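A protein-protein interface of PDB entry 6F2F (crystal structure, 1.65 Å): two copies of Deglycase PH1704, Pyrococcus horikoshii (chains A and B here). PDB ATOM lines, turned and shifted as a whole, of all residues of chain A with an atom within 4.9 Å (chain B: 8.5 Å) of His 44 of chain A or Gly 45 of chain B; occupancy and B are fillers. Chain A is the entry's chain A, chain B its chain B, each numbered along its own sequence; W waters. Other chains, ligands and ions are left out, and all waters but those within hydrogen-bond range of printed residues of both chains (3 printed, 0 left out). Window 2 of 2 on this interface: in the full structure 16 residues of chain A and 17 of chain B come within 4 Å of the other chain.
The backbone carbonyl oxygen (O) of His 44 of chain B lies within hydrogen-bond range of a ring nitrogen (ND1) of His 44 of chain A (2.9 Å). The side-chain hydroxyl of Tyr 46 of chain B is in hydrogen-bond range of the side-chain carboxylate of Glu 12 of chain A. The side-chain hydroxyl (OH) of Tyr 46 of chain A is in hydrogen-bond range of the backbone NH (N) of Val 14 of chain B (3.0 Å). N of Asp 13 of chain B sits at hydrogen-bond distance from OH of Tyr 46 of chain A (3.4 Å). The backbone NH of Asp 13 of chain A sits at hydrogen-bond distance from the side-chain hydroxyl of Tyr 46 of chain B, 3.3 Å away. The side-chain hydroxyl of Tyr 46 of chain A lies within hydrogen-bond range of the side-chain carboxylate of Glu 12 of chain B (2.6 Å).
The backbone NH (N) of His 44 of chain B is in hydrogen-bond range of the side-chain carboxylate (OD1) of Asp 13 of chain B, at 2.8 Å. The side-chain amino group of Lys 43 of chain B lies within salt-bridge range of the side-chain carboxylate of Glu 12 of chain B (2.8 Å). The side-chain carboxylate (OD1) of Asp 13 of chain A lies within hydrogen-bond range of the backbone NH (N) of His 44 of chain A (2.8 Å). OD2 of Asp 13 of chain B is in hydrogen-bond range of N of Gly 45 of chain B. The side-chain carboxylate (OE1) of Glu 12 of chain A sits close to a ring nitrogen (NE2) of His 44 of chain A (3.3 Å). OD2 of Asp 13 of chain B sits at hydrogen-bond distance from N of Tyr 46 of chain B (3.0 Å).
Among the printed residues, merely in contact across the chains: His 44 of chain A with Gly 45 of chain B (3.9 Å), His 44 of chain A with Tyr 46 of chain B (3.3 Å) and Tyr 46 of chain A with His 44 of chain B (3.3 Å).
His 44 of chain A touches just these residues of chain B: His 44, Gly 45 and Tyr 46. No residue of chain B comes within 4 Å of Gly 45 of chain A. Printed residues of chain B within 4 Å of Tyr 46 of chain A: Glu 12 (2.6 Å), Asp 13 (3.4 Å), Val 14 (3.0 Å) and His 44 (3.3 Å). Printed residues of chain A within 4 Å of Glu 12 of chain B: Tyr 46. Printed residues of chain A within 4 Å of Gly 45 of chain B: His 44 (3.9 Å). Printed residues of chain A within 4 Å of Tyr 46 of chain B: Glu 12 (2.6 Å), Asp 13 (3.3 Å) and His 44 (3.3 Å). The nearest printed residue of chain A that does not touch Tyr 46 of chain B is Tyr 46 of chain A (4.7 Å).
Printed residues of chain A that touch a printed residue of chain B: Glu 12, Asp 13, His 44 and Tyr 46. Among the printed residues, 9 pairs touch across the chains.
Glu 12 of chain A touches Tyr 46 of chain B, and with the chains exchanged Tyr 46 of chain A touches Glu 12 of chain B. Asp 13 of chain A touches Tyr 46 of chain B, and with the chains exchanged Tyr 46 of chain A touches Asp 13 of chain B. His 44 of chain A touches its own counterpart, His 44 of chain B. His 44 of chain A touches Gly 45 of chain B, but with the chains exchanged Gly 45 of chain A does not touch His 44 of chain B (4.04 Å). Positions printed for both chains: 12, 13, 42, 43, 44, 45 and 46. Of the 9 pairs that touch across the chains among the printed residues, 7 have their exchanged pair printed and touching as well.
Water W3 bridges O of His 44 of chain B (3.1 Å) and O of His 44 of chain A (3.2 Å). Water W2 bridges ND1 of His 44 of chain B (3.1 Å) and O of His 44 of chain A (3.3 Å). Water W1 bridges a ring nitrogen (ND1) of His 44 of chain A and the backbone carbonyl oxygen (O) of His 44 of chain B.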
ATOM      1  N   GLU A  12      15.571  -3.968   4.588  1.00  0.00           N
ATOM      2  CA  GLU A  12      14.740  -2.762   4.565  1.00  0.00           C
ATOM      3  C   GLU A  12      14.361  -2.548   6.032  1.00  0.00           C
ATOM      4  O   GLU A  12      13.613  -3.349   6.608  1.00  0.00           O
ATOM      5  CB  GLU A  12      13.498  -2.944   3.698  1.00  0.00           C
ATOM      6  CG  GLU A  12      12.627  -1.698   3.673  1.00  0.00           C
ATOM      7  CD  GLU A  12      13.315  -0.489   3.089  1.00  0.00           C
ATOM      8  OE1 GLU A  12      13.540   0.493   3.825  1.00  0.00           O
ATOM      9  OE2 GLU A  12      13.601  -0.499   1.876  1.00  0.00           O
ATOM     10  N   ASP A  13      14.821  -1.442   6.612  1.00  0.00           N
ATOM     11  CA  ASP A  13      14.776  -1.231   8.064  1.00  0.00           C
ATOM     12  C   ASP A  13      13.413  -1.432   8.706  1.00  0.00           C
ATOM     13  O   ASP A  13      13.287  -2.243   9.644  1.00  0.00           O
ATOM     14  CB  ASP A  13      15.371   0.097   8.475  1.00  0.00           C
ATOM     15  CG  ASP A  13      16.716   0.406   7.824  1.00  0.00           C
ATOM     16  OD1 ASP A  13      16.807   0.327   6.579  1.00  0.00           O
ATOM     17  OD2 ASP A  13      17.656   0.762   8.541  1.00  0.00           O
ATOM     18  N   GLY A  42      20.702  -1.907   8.440  1.00  0.00           N
ATOM     19  CA  GLY A  42      19.726  -1.768   7.364  1.00  0.00           C
ATOM     20  C   GLY A  42      20.165  -0.800   6.299  1.00  0.00           C
ATOM     21  O   GLY A  42      21.138  -0.069   6.467  1.00  0.00           O
ATOM     22  N   LYS A  43      19.406  -0.761   5.206  1.00  0.00           N
ATOM     23  CA  LYS A  43      19.616   0.173   4.103  1.00  0.00           C
ATOM     24  C   LYS A  43      19.662   1.615   4.602  1.00  0.00           C
ATOM     25  O   LYS A  43      20.439   2.443   4.098  1.00  0.00           O
ATOM     26  CB  LYS A  43      18.455   0.077   3.097  1.00  0.00           C
ATOM     27  CG  LYS A  43      18.510  -1.109   2.197  1.00  0.00           C
ATOM     28  CD  LYS A  43      17.178  -1.278   1.429  1.00  0.00           C
ATOM     29  CE  LYS A  43      16.760  -0.065   0.619  1.00  0.00           C
ATOM     30  NZ  LYS A  43      15.547  -0.336  -0.207  1.00  0.00           N
ATOM     31  N   HIS A  44      18.830   1.916   5.596  1.00  0.00           N
ATOM     32  CA  HIS A  44      18.711   3.265   6.169  1.00  0.00           C
ATOM     33  C   HIS A  44      19.538   3.498   7.436  1.00  0.00           C
ATOM     34  O   HIS A  44      19.424   4.554   8.051  1.00  0.00           O
ATOM     35  CB  HIS A  44      17.248   3.600   6.438  1.00  0.00           C
ATOM     36  CG  HIS A  44      16.422   3.707   5.209  1.00  0.00           C
ATOM     37  ND1 HIS A  44      16.163   4.942   4.625  1.00  0.00           N
ATOM     38  CD2 HIS A  44      15.743   2.761   4.538  1.00  0.00           C
ATOM     39  CE1 HIS A  44      15.377   4.688   3.589  1.00  0.00           C
ATOM     40  NE2 HIS A  44      15.105   3.393   3.491  1.00  0.00           N
ATOM     41  N   GLY A  45      20.393   2.555   7.801  1.00  0.00           N
ATOM     42  CA  GLY A  45      21.339   2.736   8.882  1.00  0.00           C
ATOM     43  C   GLY A  45      20.928   2.286  10.264  1.00  0.00           C
ATOM     44  O   GLY A  45      21.714   2.435  11.194  1.00  0.00           O
ATOM     45  N   TYR A  46      19.731   1.710  10.443  1.00  0.00           N
ATOM     46  CA  TYR A  46      19.387   1.176  11.761  1.00  0.00           C
ATOM     47  C   TYR A  46      20.190  -0.101  11.982  1.00  0.00           C
ATOM     48  O   TYR A  46      20.297  -0.915  11.071  1.00  0.00           O
ATOM     49  CB  TYR A  46      17.892   0.807  11.835  1.00  0.00           C
ATOM     50  CG  TYR A  46      17.012   2.003  12.077  1.00  0.00           C
ATOM     51  CD1 TYR A  46      16.777   2.461  13.356  1.00  0.00           C
ATOM     52  CD2 TYR A  46      16.337   2.625  11.029  1.00  0.00           C
ATOM     53  CE1 TYR A  46      15.983   3.575  13.586  1.00  0.00           C
ATOM     54  CE2 TYR A  46      15.512   3.716  11.249  1.00  0.00           C
ATOM     55  CZ  TYR A  46      15.299   4.160  12.536  1.00  0.00           C
ATOM     56  OH  TYR A  46      14.469   5.240  12.743  1.00  0.00           O
ATOM     57  N   GLU B  10      13.553  15.513  10.191  1.00  0.00           N
ATOM     58  CA  GLU B  10      14.455  14.951  11.190  1.00  0.00           C
ATOM     59  C   GLU B  10      13.697  14.262  12.311  1.00  0.00           C
ATOM     60  O   GLU B  10      14.223  14.042  13.393  1.00  0.00           O
ATOM     61  CB  GLU B  10      15.493  15.953  11.700  1.00  0.00           C
ATOM     62  CG  GLU B  10      16.281  16.605  10.574  1.00  0.00           C
ATOM     63  CD  GLU B  10      17.054  15.652   9.682  1.00  0.00           C
ATOM     64  OE1 GLU B  10      17.020  15.818   8.440  1.00  0.00           O
ATOM     65  OE2 GLU B  10      17.668  14.711  10.229  1.00  0.00           O
ATOM     66  N   PHE B  11      12.473  13.802  12.018  1.00  0.00           N
ATOM     67  CA  PHE B  11      11.798  12.920  12.936  1.00  0.00           C
ATOM     68  C   PHE B  11      12.565  11.587  13.016  1.00  0.00           C
ATOM     69  O   PHE B  11      13.266  11.215  12.076  1.00  0.00           O
ATOM     70  CB  PHE B  11      10.340  12.658  12.441  1.00  0.00           C
ATOM     71  CG  PHE B  11      10.174  11.988  11.075  1.00  0.00           C
ATOM     72  CD1 PHE B  11      10.143  10.600  10.957  1.00  0.00           C
ATOM     73  CD2 PHE B  11      10.040  12.740   9.920  1.00  0.00           C
ATOM     74  CE1 PHE B  11       9.974   9.994   9.718  1.00  0.00           C
ATOM     75  CE2 PHE B  11       9.852  12.125   8.681  1.00  0.00           C
ATOM     76  CZ  PHE B  11       9.898  10.755   8.574  1.00  0.00           C
ATOM     77  N   GLU B  12      12.442  10.888  14.136  1.00  0.00           N
ATOM     78  CA  GLU B  12      13.055   9.564  14.283  1.00  0.00           C
ATOM     79  C   GLU B  12      12.144   8.642  13.468  1.00  0.00           C
ATOM     80  O   GLU B  12      10.961   8.474  13.787  1.00  0.00           O
ATOM     81  CB  GLU B  12      13.133   9.134  15.748  1.00  0.00           C
ATOM     82  CG  GLU B  12      13.756   7.764  15.910  1.00  0.00           C
ATOM     83  CD  GLU B  12      15.184   7.698  15.437  1.00  0.00           C
ATOM     84  OE1 GLU B  12      16.034   8.414  16.001  1.00  0.00           O
ATOM     85  OE2 GLU B  12      15.448   6.958  14.473  1.00  0.00           O
ATOM     86  N   ASP B  13      12.668   8.065  12.392  1.00  0.00           N
ATOM     87  CA  ASP B  13      11.853   7.377  11.405  1.00  0.00           C
ATOM     88  C   ASP B  13      10.901   6.335  11.941  1.00  0.00           C
ATOM     89  O   ASP B  13       9.695   6.393  11.665  1.00  0.00           O
ATOM     90  CB  ASP B  13      12.700   6.804  10.271  1.00  0.00           C
ATOM     91  CG  ASP B  13      13.731   7.784   9.719  1.00  0.00           C
ATOM     92  OD1 ASP B  13      14.514   8.342  10.522  1.00  0.00           O
ATOM     93  OD2 ASP B  13      13.812   7.931   8.496  1.00  0.00           O
ATOM     94  N   VAL B  14      11.427   5.366  12.691  1.00  0.00           N
ATOM     95  CA  VAL B  14      10.575   4.293  13.196  1.00  0.00           C
ATOM     96  C   VAL B  14       9.580   4.781  14.239  1.00  0.00           C
ATOM     97  O   VAL B  14       8.494   4.194  14.375  1.00  0.00           O
ATOM     98  CB  VAL B  14      11.361   3.075  13.706  1.00  0.00           C
ATOM     99  CG1 VAL B  14      12.147   2.429  12.577  1.00  0.00           C
ATOM    100  CG2 VAL B  14      12.261   3.412  14.898  1.00  0.00           C
ATOM    101  N   ILE B  17       6.809   5.928  11.784  1.00  0.00           N
ATOM    102  CA  ILE B  17       6.279   4.863  10.936  1.00  0.00           C
ATOM    103  C   ILE B  17       5.620   3.718  11.724  1.00  0.00           C
ATOM    104  O   ILE B  17       4.540   3.236  11.321  1.00  0.00           O
ATOM    105  CB  ILE B  17       7.384   4.350   9.970  1.00  0.00           C
ATOM    106  CG1 ILE B  17       7.805   5.486   9.008  1.00  0.00           C
ATOM    107  CG2 ILE B  17       6.916   3.113   9.197  1.00  0.00           C
ATOM    108  CD1 ILE B  17       9.145   5.233   8.314  1.00  0.00           C
ATOM    109  N   ILE B  40       8.189  15.271   4.279  1.00  0.00           N
ATOM    110  CA  ILE B  40       9.186  15.459   5.318  1.00  0.00           C
ATOM    111  C   ILE B  40      10.049  14.217   5.297  1.00  0.00           C
ATOM    112  O   ILE B  40       9.588  13.168   4.865  1.00  0.00           O
ATOM    113  CB  ILE B  40       8.636  15.739   6.700  1.00  0.00           C
ATOM    114  CG1 ILE B  40       7.538  14.733   7.056  1.00  0.00           C
ATOM    115  CG2 ILE B  40       8.124  17.193   6.722  1.00  0.00           C
ATOM    116  CD1 ILE B  40       7.000  14.877   8.496  1.00  0.00           C
ATOM    117  N   THR B  41      11.310  14.343   5.760  1.00  0.00           N
ATOM    118  CA  THR B  41      12.288  13.260   5.717  1.00  0.00           C
ATOM    119  C   THR B  41      12.838  13.023   7.095  1.00  0.00           C
ATOM    120  O   THR B  41      13.210  13.969   7.794  1.00  0.00           O
ATOM    121  CB  THR B  41      13.399  13.610   4.720  1.00  0.00           C
ATOM    122  OG1 THR B  41      12.800  13.881   3.443  1.00  0.00           O
ATOM    123  CG2 THR B  41      14.413  12.475   4.543  1.00  0.00           C
ATOM    124  N   GLY B  42      12.923  11.753   7.483  1.00  0.00           N
ATOM    125  CA  GLY B  42      13.409  11.384   8.798  1.00  0.00           C
ATOM    126  C   GLY B  42      14.913  11.482   8.895  1.00  0.00           C
ATOM    127  O   GLY B  42      15.616  11.594   7.880  1.00  0.00           O
ATOM    128  N   LYS B  43      15.416  11.329  10.110  1.00  0.00           N
ATOM    129  CA  LYS B  43      16.853  11.282  10.392  1.00  0.00           C
ATOM    130  C   LYS B  43      17.556  10.232   9.520  1.00  0.00           C
ATOM    131  O   LYS B  43      18.695  10.434   9.072  1.00  0.00           O
ATOM    132  CB  LYS B  43      17.105  10.895  11.854  1.00  0.00           C
ATOM    133  CG  LYS B  43      16.863  12.008  12.828  1.00  0.00           C
ATOM    134  CD  LYS B  43      16.855  11.467  14.281  1.00  0.00           C
ATOM    135  CE  LYS B  43      18.108  10.720  14.682  1.00  0.00           C
ATOM    136  NZ  LYS B  43      18.096  10.344  16.125  1.00  0.00           N
ATOM    137  N   HIS B  44      16.880   9.099   9.311  1.00  0.00           N
ATOM    138  CA  HIS B  44      17.405   7.966   8.536  1.00  0.00           C
ATOM    139  C   HIS B  44      16.987   7.932   7.083  1.00  0.00           C
ATOM    140  O   HIS B  44      17.299   6.971   6.374  1.00  0.00           O
ATOM    141  CB  HIS B  44      17.039   6.638   9.212  1.00  0.00           C
ATOM    142  CG  HIS B  44      17.669   6.451  10.540  1.00  0.00           C
ATOM    143  ND1 HIS B  44      18.821   5.702  10.683  1.00  0.00           N
ATOM    144  CD2 HIS B  44      17.240   6.832  11.758  1.00  0.00           C
ATOM    145  CE1 HIS B  44      19.080   5.692  11.982  1.00  0.00           C
ATOM    146  NE2 HIS B  44      18.171   6.360  12.669  1.00  0.00           N
ATOM    147  N   GLY B  45      16.360   8.982   6.594  1.00  0.00           N
ATOM    148  CA  GLY B  45      16.073   9.119   5.174  1.00  0.00           C
ATOM    149  C   GLY B  45      14.738   8.620   4.673  1.00  0.00           C
ATOM    150  O   GLY B  45      14.487   8.716   3.479  1.00  0.00           O
ATOM    151  N   TYR B  46      13.870   8.098   5.525  1.00  0.00           N
ATOM    152  CA  TYR B  46      12.530   7.727   5.049  1.00  0.00           C
ATOM    153  C   TYR B  46      11.734   9.012   4.808  1.00  0.00           C
ATOM    154  O   TYR B  46      11.778   9.914   5.635  1.00  0.00           O
ATOM    155  CB  TYR B  46      11.768   6.914   6.109  1.00  0.00           C
ATOM    156  CG  TYR B  46      12.163   5.463   6.122  1.00  0.00           C
ATOM    157  CD1 TYR B  46      11.580   4.561   5.253  1.00  0.00           C
ATOM    158  CD2 TYR B  46      13.088   4.980   7.042  1.00  0.00           C
ATOM    159  CE1 TYR B  46      11.979   3.226   5.225  1.00  0.00           C
ATOM    160  CE2 TYR B  46      13.445   3.637   7.072  1.00  0.00           C
ATOM    161  CZ  TYR B  46      12.855   2.750   6.190  1.00  0.00           C
ATOM    162  OH  TYR B  46      13.208   1.414   6.241  1.00  0.00           O
ATOM    163  N   SER B  47      10.995   9.069   3.683  1.00  0.00           N
ATOM    164  CA  SER B  47      10.166  10.233   3.352  1.00  0.00           C
ATOM    165  C   SER B  47       8.708   9.890   3.572  1.00  0.00           C
ATOM    166  O   SER B  47       8.278   8.797   3.224  1.00  0.00           O
ATOM    167  CB  SER B  47      10.378  10.678   1.907  1.00  0.00           C
ATOM    168  OG  SER B  47       9.944   9.711   0.974  1.00  0.00           O
ATOM    169  N   VAL B  48       7.953  10.821   4.144  1.00  0.00           N
ATOM    170  CA  VAL B  48       6.520  10.636   4.351  1.00  0.00           C
ATOM    171  C   VAL B  48       5.809  11.873   3.865  1.00  0.00           C
ATOM    172  O   VAL B  48       6.337  12.984   3.931  1.00  0.00           O
ATOM    173  CB  VAL B  48       6.122  10.260   5.797  1.00  0.00           C
ATOM    174  CG1 VAL B  48       6.929   9.078   6.296  1.00  0.00           C
ATOM    175  CG2 VAL B  48       6.282  11.403   6.720  1.00  0.00           C
HETATM  176  O   HOH W   1      18.681   6.617   3.374  1.00  0.00           O
HETATM  177  O   HOH W   2      21.659   6.514   9.593  1.00  0.00           O
HETATM  178  O   HOH W   3      20.332   6.816   5.948  1.00  0.00           O
